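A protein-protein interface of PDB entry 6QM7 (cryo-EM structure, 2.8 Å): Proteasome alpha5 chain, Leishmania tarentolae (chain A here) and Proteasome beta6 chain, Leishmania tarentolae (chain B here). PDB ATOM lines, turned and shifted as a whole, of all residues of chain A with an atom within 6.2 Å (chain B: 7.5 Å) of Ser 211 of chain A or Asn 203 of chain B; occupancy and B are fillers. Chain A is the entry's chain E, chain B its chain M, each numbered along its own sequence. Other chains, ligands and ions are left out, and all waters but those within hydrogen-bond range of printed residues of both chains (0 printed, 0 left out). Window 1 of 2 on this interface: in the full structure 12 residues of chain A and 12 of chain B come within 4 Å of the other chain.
The side-chain amide oxygen (OD1) of Asn 204 of chain B sits at hydrogen-bond distance from the side-chain hydroxyl (OG) of Ser 208 of chain A. The backbone NH of Gly 205 of chain B sits close to the side-chain carboxylate of Glu 210 of chain A (3.4 Å).
The backbone carbonyl oxygen (O) of Trp 199 of chain B is in hydrogen-bond range of the side-chain amide nitrogen (ND2) of Asn 203 of chain B, 3.0 Å away. OH of Tyr 200 of chain B sits at hydrogen-bond distance from NZ of Lys 207 of chain B (3.1 Å). OG of Ser 208 of chain A lies close to N of Ser 211 of chain A (3.2 Å). The backbone carbonyl oxygen of Tyr 200 of chain B lies within hydrogen-bond range of the side-chain amide nitrogen of Asn 204 of chain B, 2.9 Å away.
Among the printed residues, merely in contact across the chains: Leu 214 of chain A with Asn 203 of chain B (3.4 Å), Ser 211 of chain A with Asn 203 of chain B (3.4 Å), Ser 211 of chain A with Asn 204 of chain B (3.5 Å), His 199 of chain A with Tyr 200 of chain B (3.7 Å), His 199 of chain A with Asn 204 of chain B (3.8 Å) and Glu 210 of chain A with Asn 204 of chain B (3.9 Å).
Of the printed residues of chain B, His 199 of chain A touches Tyr 200 (3.7 Å) and Asn 204 (3.8 Å). Of the printed residues of chain B, Glu 210 of chain A touches Asn 204 (3.9 Å) and Gly 205 (3.3 Å). Of chain B, only Asn 203 and Asn 204 come within 4 Å of Ser 211 of chain A. Of the printed residues of chain A, Tyr 200 of chain B touches His 199 (3.7 Å). Printed residues of chain A within 4 Å of Asn 203 of chain B: Ser 211 (3.4 Å) and Leu 214 (3.4 Å). Printed residues of chain A within 4 Å of Asn 204 of chain B: His 199, Ser 208, Glu 210 and Ser 211. Of the printed residues of chain A, Gly 205 of chain B touches Glu 210 (3.3 Å). The nearest residue of chain B that does not touch Ser 211 of chain A is Gly 205 of chain B (6.3 Å). The nearest residue of chain A that does not touch Asn 203 of chain B is Ser 208 of chain A (4.4 Å).
Of the 12 printed residues of chain B, 4 touch a printed residue of chain A. Hydrophobic or aromatic side chains of chain B within 4 Å of the printed part of chain A: Tyr 200. Among the printed residues, no Asp or Glu carboxylate lies within 4 Å of a Lys or Arg side-chain nitrogen of the other chain.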
ATOM      1  N   GLU A 195       5.139 -32.601   3.405  1.00  0.00           N
ATOM      2  CA  GLU A 195       6.140 -31.541   3.123  1.00  0.00           C
ATOM      3  C   GLU A 195       5.444 -30.341   2.474  1.00  0.00           C
ATOM      4  O   GLU A 195       5.732 -29.215   2.899  1.00  0.00           O
ATOM      5  CB  GLU A 195       7.293 -32.108   2.293  1.00  0.00           C
ATOM      6  CG  GLU A 195       8.119 -33.128   3.071  1.00  0.00           C
ATOM      7  CD  GLU A 195       8.972 -32.574   4.214  1.00  0.00           C
ATOM      8  OE1 GLU A 195      10.218 -32.521   4.050  1.00  0.00           O
ATOM      9  OE2 GLU A 195       8.399 -32.215   5.279  1.00  0.00           O
ATOM     10  N   HIS A 199       5.213 -26.708   4.079  1.00  0.00           N
ATOM     11  CA  HIS A 199       5.654 -25.515   3.326  1.00  0.00           C
ATOM     12  C   HIS A 199       4.594 -24.435   3.461  1.00  0.00           C
ATOM     13  O   HIS A 199       4.954 -23.330   3.868  1.00  0.00           O
ATOM     14  CB  HIS A 199       5.945 -25.825   1.855  1.00  0.00           C
ATOM     15  CG  HIS A 199       6.750 -24.753   1.219  1.00  0.00           C
ATOM     16  ND1 HIS A 199       8.125 -24.769   1.240  1.00  0.00           N
ATOM     17  CD2 HIS A 199       6.379 -23.593   0.633  1.00  0.00           C
ATOM     18  CE1 HIS A 199       8.572 -23.679   0.642  1.00  0.00           C
ATOM     19  NE2 HIS A 199       7.521 -22.942   0.253  1.00  0.00           N
ATOM     20  N   MET A 207       4.010 -24.798  -2.046  1.00  0.00           N
ATOM     21  CA  MET A 207       5.358 -25.354  -2.288  1.00  0.00           C
ATOM     22  C   MET A 207       5.615 -25.339  -3.793  1.00  0.00           C
ATOM     23  O   MET A 207       4.688 -25.645  -4.565  1.00  0.00           O
ATOM     24  CB  MET A 207       5.459 -26.791  -1.772  1.00  0.00           C
ATOM     25  CG  MET A 207       6.871 -27.232  -1.520  1.00  0.00           C
ATOM     26  SD  MET A 207       6.939 -28.831  -0.696  1.00  0.00           S
ATOM     27  CE  MET A 207       8.515 -28.704   0.151  1.00  0.00           C
ATOM     28  N   SER A 208       6.830 -24.982  -4.189  1.00  0.00           N
ATOM     29  CA  SER A 208       7.289 -25.115  -5.587  1.00  0.00           C
ATOM     30  C   SER A 208       7.264 -26.600  -5.955  1.00  0.00           C
ATOM     31  O   SER A 208       7.356 -27.423  -5.036  1.00  0.00           O
ATOM     32  CB  SER A 208       8.645 -24.482  -5.774  1.00  0.00           C
ATOM     33  OG  SER A 208       9.652 -25.140  -5.025  1.00  0.00           O
ATOM     34  N   VAL A 209       7.112 -26.932  -7.238  1.00  0.00           N
ATOM     35  CA  VAL A 209       7.066 -28.350  -7.696  1.00  0.00           C
ATOM     36  C   VAL A 209       8.433 -28.996  -7.460  1.00  0.00           C
ATOM     37  O   VAL A 209       8.468 -30.144  -7.003  1.00  0.00           O
ATOM     38  CB  VAL A 209       6.679 -28.478  -9.176  1.00  0.00           C
ATOM     39  CG1 VAL A 209       6.619 -29.935  -9.610  1.00  0.00           C
ATOM     40  CG2 VAL A 209       5.369 -27.771  -9.474  1.00  0.00           C
ATOM     41  N   GLU A 210       9.505 -28.290  -7.813  1.00  0.00           N
ATOM     42  CA  GLU A 210      10.910 -28.722  -7.592  1.00  0.00           C
ATOM     43  C   GLU A 210      11.147 -29.011  -6.101  1.00  0.00           C
ATOM     44  O   GLU A 210      11.724 -30.064  -5.804  1.00  0.00           O
ATOM     45  CB  GLU A 210      11.851 -27.632  -8.102  1.00  0.00           C
ATOM     46  CG  GLU A 210      13.328 -27.933  -7.915  1.00  0.00           C
ATOM     47  CD  GLU A 210      14.242 -26.852  -8.473  1.00  0.00           C
ATOM     48  OE1 GLU A 210      13.867 -25.662  -8.366  1.00  0.00           O
ATOM     49  OE2 GLU A 210      15.323 -27.196  -9.023  1.00  0.00           O
ATOM     50  N   SER A 211      10.742 -28.109  -5.201  1.00  0.00           N
ATOM     51  CA  SER A 211      10.927 -28.253  -3.729  1.00  0.00           C
ATOM     52  C   SER A 211      10.200 -29.504  -3.228  1.00  0.00           C
ATOM     53  O   SER A 211      10.728 -30.186  -2.336  1.00  0.00           O
ATOM     54  CB  SER A 211      10.470 -27.022  -2.975  1.00  0.00           C
ATOM     55  OG  SER A 211      10.707 -27.138  -1.580  1.00  0.00           O
ATOM     56  N   CYS A 212       9.031 -29.782  -3.790  1.00  0.00           N
ATOM     57  CA  CYS A 212       8.185 -30.950  -3.454  1.00  0.00           C
ATOM     58  C   CYS A 212       8.818 -32.228  -4.001  1.00  0.00           C
ATOM     59  O   CYS A 212       8.713 -33.270  -3.353  1.00  0.00           O
ATOM     60  CB  CYS A 212       6.786 -30.785  -4.031  1.00  0.00           C
ATOM     61  SG  CYS A 212       5.650 -32.044  -3.414  1.00  0.00           S
ATOM     62  N   THR A 213       9.418 -32.156  -5.175  1.00  0.00           N
ATOM     63  CA  THR A 213      10.178 -33.282  -5.759  1.00  0.00           C
ATOM     64  C   THR A 213      11.380 -33.577  -4.855  1.00  0.00           C
ATOM     65  O   THR A 213      11.552 -34.749  -4.497  1.00  0.00           O
ATOM     66  CB  THR A 213      10.558 -32.991  -7.217  1.00  0.00           C
ATOM     67  OG1 THR A 213       9.431 -32.443  -7.903  1.00  0.00           O
ATOM     68  CG2 THR A 213      10.989 -34.242  -7.940  1.00  0.00           C
ATOM     69  N   LEU A 214      12.163 -32.550  -4.514  1.00  0.00           N
ATOM     70  CA  LEU A 214      13.377 -32.642  -3.655  1.00  0.00           C
ATOM     71  C   LEU A 214      13.037 -33.291  -2.316  1.00  0.00           C
ATOM     72  O   LEU A 214      13.821 -34.124  -1.876  1.00  0.00           O
ATOM     73  CB  LEU A 214      13.963 -31.252  -3.400  1.00  0.00           C
ATOM     74  CG  LEU A 214      14.917 -30.732  -4.471  1.00  0.00           C
ATOM     75  CD1 LEU A 214      15.159 -29.232  -4.311  1.00  0.00           C
ATOM     76  CD2 LEU A 214      16.229 -31.479  -4.414  1.00  0.00           C
ATOM     77  N   ALA A 215      11.933 -32.893  -1.693  1.00  0.00           N
ATOM     78  CA  ALA A 215      11.462 -33.410  -0.384  1.00  0.00           C
ATOM     79  C   ALA A 215      11.060 -34.886  -0.498  1.00  0.00           C
ATOM     80  O   ALA A 215      11.293 -35.626   0.454  1.00  0.00           O
ATOM     81  CB  ALA A 215      10.314 -32.572   0.127  1.00  0.00           C
ATOM     82  N   THR A 216      10.457 -35.282  -1.615  1.00  0.00           N
ATOM     83  CA  THR A 216      10.072 -36.682  -1.940  1.00  0.00           C
ATOM     84  C   THR A 216      11.329 -37.535  -2.129  1.00  0.00           C
ATOM     85  O   THR A 216      11.299 -38.721  -1.770  1.00  0.00           O
ATOM     86  CB  THR A 216       9.159 -36.708  -3.172  1.00  0.00           C
ATOM     87  OG1 THR A 216       7.945 -36.049  -2.809  1.00  0.00           O
ATOM     88  CG2 THR A 216       8.859 -38.105  -3.664  1.00  0.00           C
ATOM     89  N   ARG B 196      17.440 -19.808   7.233  1.00  0.00           N
ATOM     90  CA  ARG B 196      16.170 -20.352   6.698  1.00  0.00           C
ATOM     91  C   ARG B 196      15.937 -19.797   5.298  1.00  0.00           C
ATOM     92  O   ARG B 196      15.472 -20.558   4.437  1.00  0.00           O
ATOM     93  CB  ARG B 196      15.000 -20.043   7.632  1.00  0.00           C
ATOM     94  CG  ARG B 196      15.003 -20.890   8.896  1.00  0.00           C
ATOM     95  CD  ARG B 196      14.633 -22.342   8.643  1.00  0.00           C
ATOM     96  NE  ARG B 196      13.492 -22.678   9.490  1.00  0.00           N
ATOM     97  CZ  ARG B 196      12.250 -22.947   9.074  1.00  0.00           C
ATOM     98  NH1 ARG B 196      11.937 -22.983   7.786  1.00  0.00           N
ATOM     99  NH2 ARG B 196      11.309 -23.203   9.971  1.00  0.00           N
ATOM    100  N   VAL B 197      16.274 -18.537   5.073  1.00  0.00           N
ATOM    101  CA  VAL B 197      16.087 -17.870   3.760  1.00  0.00           C
ATOM    102  C   VAL B 197      17.089 -18.426   2.757  1.00  0.00           C
ATOM    103  O   VAL B 197      16.728 -18.531   1.567  1.00  0.00           O
ATOM    104  CB  VAL B 197      16.192 -16.344   3.873  1.00  0.00           C
ATOM    105  CG1 VAL B 197      16.253 -15.679   2.503  1.00  0.00           C
ATOM    106  CG2 VAL B 197      15.030 -15.788   4.676  1.00  0.00           C
ATOM    107  N   LYS B 198      18.302 -18.735   3.208  1.00  0.00           N
ATOM    108  CA  LYS B 198      19.365 -19.311   2.349  1.00  0.00           C
ATOM    109  C   LYS B 198      18.921 -20.706   1.905  1.00  0.00           C
ATOM    110  O   LYS B 198      19.029 -21.002   0.707  1.00  0.00           O
ATOM    111  CB  LYS B 198      20.690 -19.304   3.107  1.00  0.00           C
ATOM    112  CG  LYS B 198      21.899 -19.722   2.287  1.00  0.00           C
ATOM    113  CD  LYS B 198      23.092 -18.766   2.358  1.00  0.00           C
ATOM    114  CE  LYS B 198      23.151 -17.807   1.180  1.00  0.00           C
ATOM    115  NZ  LYS B 198      24.431 -17.923   0.438  1.00  0.00           N
ATOM    116  N   TRP B 199      18.396 -21.512   2.829  1.00  0.00           N
ATOM    117  CA  TRP B 199      17.878 -22.879   2.557  1.00  0.00           C
ATOM    118  C   TRP B 199      16.745 -22.811   1.540  1.00  0.00           C
ATOM    119  O   TRP B 199      16.705 -23.641   0.630  1.00  0.00           O
ATOM    120  CB  TRP B 199      17.422 -23.586   3.843  1.00  0.00           C
ATOM    121  CG  TRP B 199      18.565 -24.202   4.578  1.00  0.00           C
ATOM    122  CD1 TRP B 199      18.993 -23.930   5.841  1.00  0.00           C
ATOM    123  CD2 TRP B 199      19.486 -25.153   4.036  1.00  0.00           C
ATOM    124  NE1 TRP B 199      20.110 -24.661   6.132  1.00  0.00           N
ATOM    125  CE2 TRP B 199      20.434 -25.423   5.042  1.00  0.00           C
ATOM    126  CE3 TRP B 199      19.592 -25.808   2.803  1.00  0.00           C
ATOM    127  CZ2 TRP B 199      21.475 -26.328   4.851  1.00  0.00           C
ATOM    128  CZ3 TRP B 199      20.624 -26.697   2.613  1.00  0.00           C
ATOM    129  CH2 TRP B 199      21.548 -26.953   3.627  1.00  0.00           C
ATOM    130  N   TYR B 200      15.834 -21.872   1.729  1.00  0.00           N
ATOM    131  CA  TYR B 200      14.702 -21.648   0.805  1.00  0.00           C
ATOM    132  C   TYR B 200      15.268 -21.399  -0.592  1.00  0.00           C
ATOM    133  O   TYR B 200      14.723 -21.999  -1.512  1.00  0.00           O
ATOM    134  CB  TYR B 200      13.817 -20.519   1.326  1.00  0.00           C
ATOM    135  CG  TYR B 200      12.580 -20.275   0.504  1.00  0.00           C
ATOM    136  CD1 TYR B 200      11.329 -20.683   0.945  1.00  0.00           C
ATOM    137  CD2 TYR B 200      12.660 -19.610  -0.709  1.00  0.00           C
ATOM    138  CE1 TYR B 200      10.192 -20.432   0.198  1.00  0.00           C
ATOM    139  CE2 TYR B 200      11.533 -19.359  -1.469  1.00  0.00           C
ATOM    140  CZ  TYR B 200      10.296 -19.769  -1.012  1.00  0.00           C
ATOM    141  OH  TYR B 200       9.192 -19.503  -1.760  1.00  0.00           O
ATOM    142  N   LYS B 201      16.313 -20.581  -0.746  1.00  0.00           N
ATOM    143  CA  LYS B 201      16.905 -20.285  -2.078  1.00  0.00           C
ATOM    144  C   LYS B 201      17.348 -21.593  -2.738  1.00  0.00           C
ATOM    145  O   LYS B 201      17.129 -21.744  -3.944  1.00  0.00           O
ATOM    146  CB  LYS B 201      18.095 -19.321  -2.009  1.00  0.00           C
ATOM    147  CG  LYS B 201      17.730 -17.843  -1.963  1.00  0.00           C
ATOM    148  CD  LYS B 201      18.861 -16.968  -1.440  1.00  0.00           C
ATOM    149  CE  LYS B 201      18.852 -15.554  -1.986  1.00  0.00           C
ATOM    150  NZ  LYS B 201      19.470 -15.488  -3.333  1.00  0.00           N
ATOM    151  N   TYR B 202      17.961 -22.490  -1.972  1.00  0.00           N
ATOM    152  CA  TYR B 202      18.550 -23.758  -2.467  1.00  0.00           C
ATOM    153  C   TYR B 202      17.431 -24.737  -2.828  1.00  0.00           C
ATOM    154  O   TYR B 202      17.433 -25.271  -3.962  1.00  0.00           O
ATOM    155  CB  TYR B 202      19.501 -24.336  -1.415  1.00  0.00           C
ATOM    156  CG  TYR B 202      20.722 -23.502  -1.090  1.00  0.00           C
ATOM    157  CD1 TYR B 202      21.327 -22.695  -2.042  1.00  0.00           C
ATOM    158  CD2 TYR B 202      21.318 -23.572   0.164  1.00  0.00           C
ATOM    159  CE1 TYR B 202      22.456 -21.955  -1.744  1.00  0.00           C
ATOM    160  CE2 TYR B 202      22.459 -22.849   0.472  1.00  0.00           C
ATOM    161  CZ  TYR B 202      23.030 -22.032  -0.488  1.00  0.00           C
ATOM    162  OH  TYR B 202      24.141 -21.286  -0.219  1.00  0.00           O
ATOM    163  N   ASN B 203      16.483 -24.932  -1.910  1.00  0.00           N
ATOM    164  CA  ASN B 203      15.357 -25.888  -2.065  1.00  0.00           C
ATOM    165  C   ASN B 203      14.363 -25.394  -3.130  1.00  0.00           C
ATOM    166  O   ASN B 203      13.700 -26.253  -3.730  1.00  0.00           O
ATOM    167  CB  ASN B 203      14.665 -26.175  -0.731  1.00  0.00           C
ATOM    168  CG  ASN B 203      15.612 -26.685   0.340  1.00  0.00           C
ATOM    169  OD1 ASN B 203      16.509 -27.487   0.077  1.00  0.00           O
ATOM    170  ND2 ASN B 203      15.422 -26.216   1.564  1.00  0.00           N
ATOM    171  N   ASN B 204      14.256 -24.081  -3.374  1.00  0.00           N
ATOM    172  CA  ASN B 204      13.293 -23.494  -4.352  1.00  0.00           C
ATOM    173  C   ASN B 204      14.075 -22.918  -5.537  1.00  0.00           C
ATOM    174  O   ASN B 204      13.674 -21.870  -6.047  1.00  0.00           O
ATOM    175  CB  ASN B 204      12.343 -22.493  -3.684  1.00  0.00           C
ATOM    176  CG  ASN B 204      11.541 -23.109  -2.551  1.00  0.00           C
ATOM    177  OD1 ASN B 204      10.385 -23.499  -2.733  1.00  0.00           O
ATOM    178  ND2 ASN B 204      12.140 -23.213  -1.374  1.00  0.00           N
ATOM    179  N   GLY B 205      15.136 -23.611  -5.960  1.00  0.00           N
ATOM    180  CA  GLY B 205      15.919 -23.334  -7.181  1.00  0.00           C
ATOM    181  C   GLY B 205      16.190 -21.860  -7.420  1.00  0.00           C
ATOM    182  O   GLY B 205      15.701 -21.334  -8.440  1.00  0.00           O
ATOM    183  N   GLY B 206      16.933 -21.215  -6.518  1.00  0.00           N
ATOM    184  CA  GLY B 206      17.421 -19.828  -6.673  1.00  0.00           C
ATOM    185  C   GLY B 206      16.412 -18.778  -6.236  1.00  0.00           C
ATOM    186  O   GLY B 206      16.854 -17.682  -5.847  1.00  0.00           O
ATOM    187  N   LYS B 207      15.113 -19.091  -6.313  1.00  0.00           N
ATOM    188  CA  LYS B 207      13.983 -18.173  -6.007  1.00  0.00           C
ATOM    189  C   LYS B 207      14.104 -17.705  -4.554  1.00  0.00           C
ATOM    190  O   LYS B 207      14.237 -18.547  -3.662  1.00  0.00           O
ATOM    191  CB  LYS B 207      12.639 -18.875  -6.244  1.00  0.00           C
ATOM    192  CG  LYS B 207      11.379 -18.036  -6.043  1.00  0.00           C
ATOM    193  CD  LYS B 207      10.140 -18.875  -5.742  1.00  0.00           C
ATOM    194  CE  LYS B 207       9.162 -18.174  -4.823  1.00  0.00           C
ATOM    195  NZ  LYS B 207       7.966 -19.009  -4.546  1.00  0.00           N
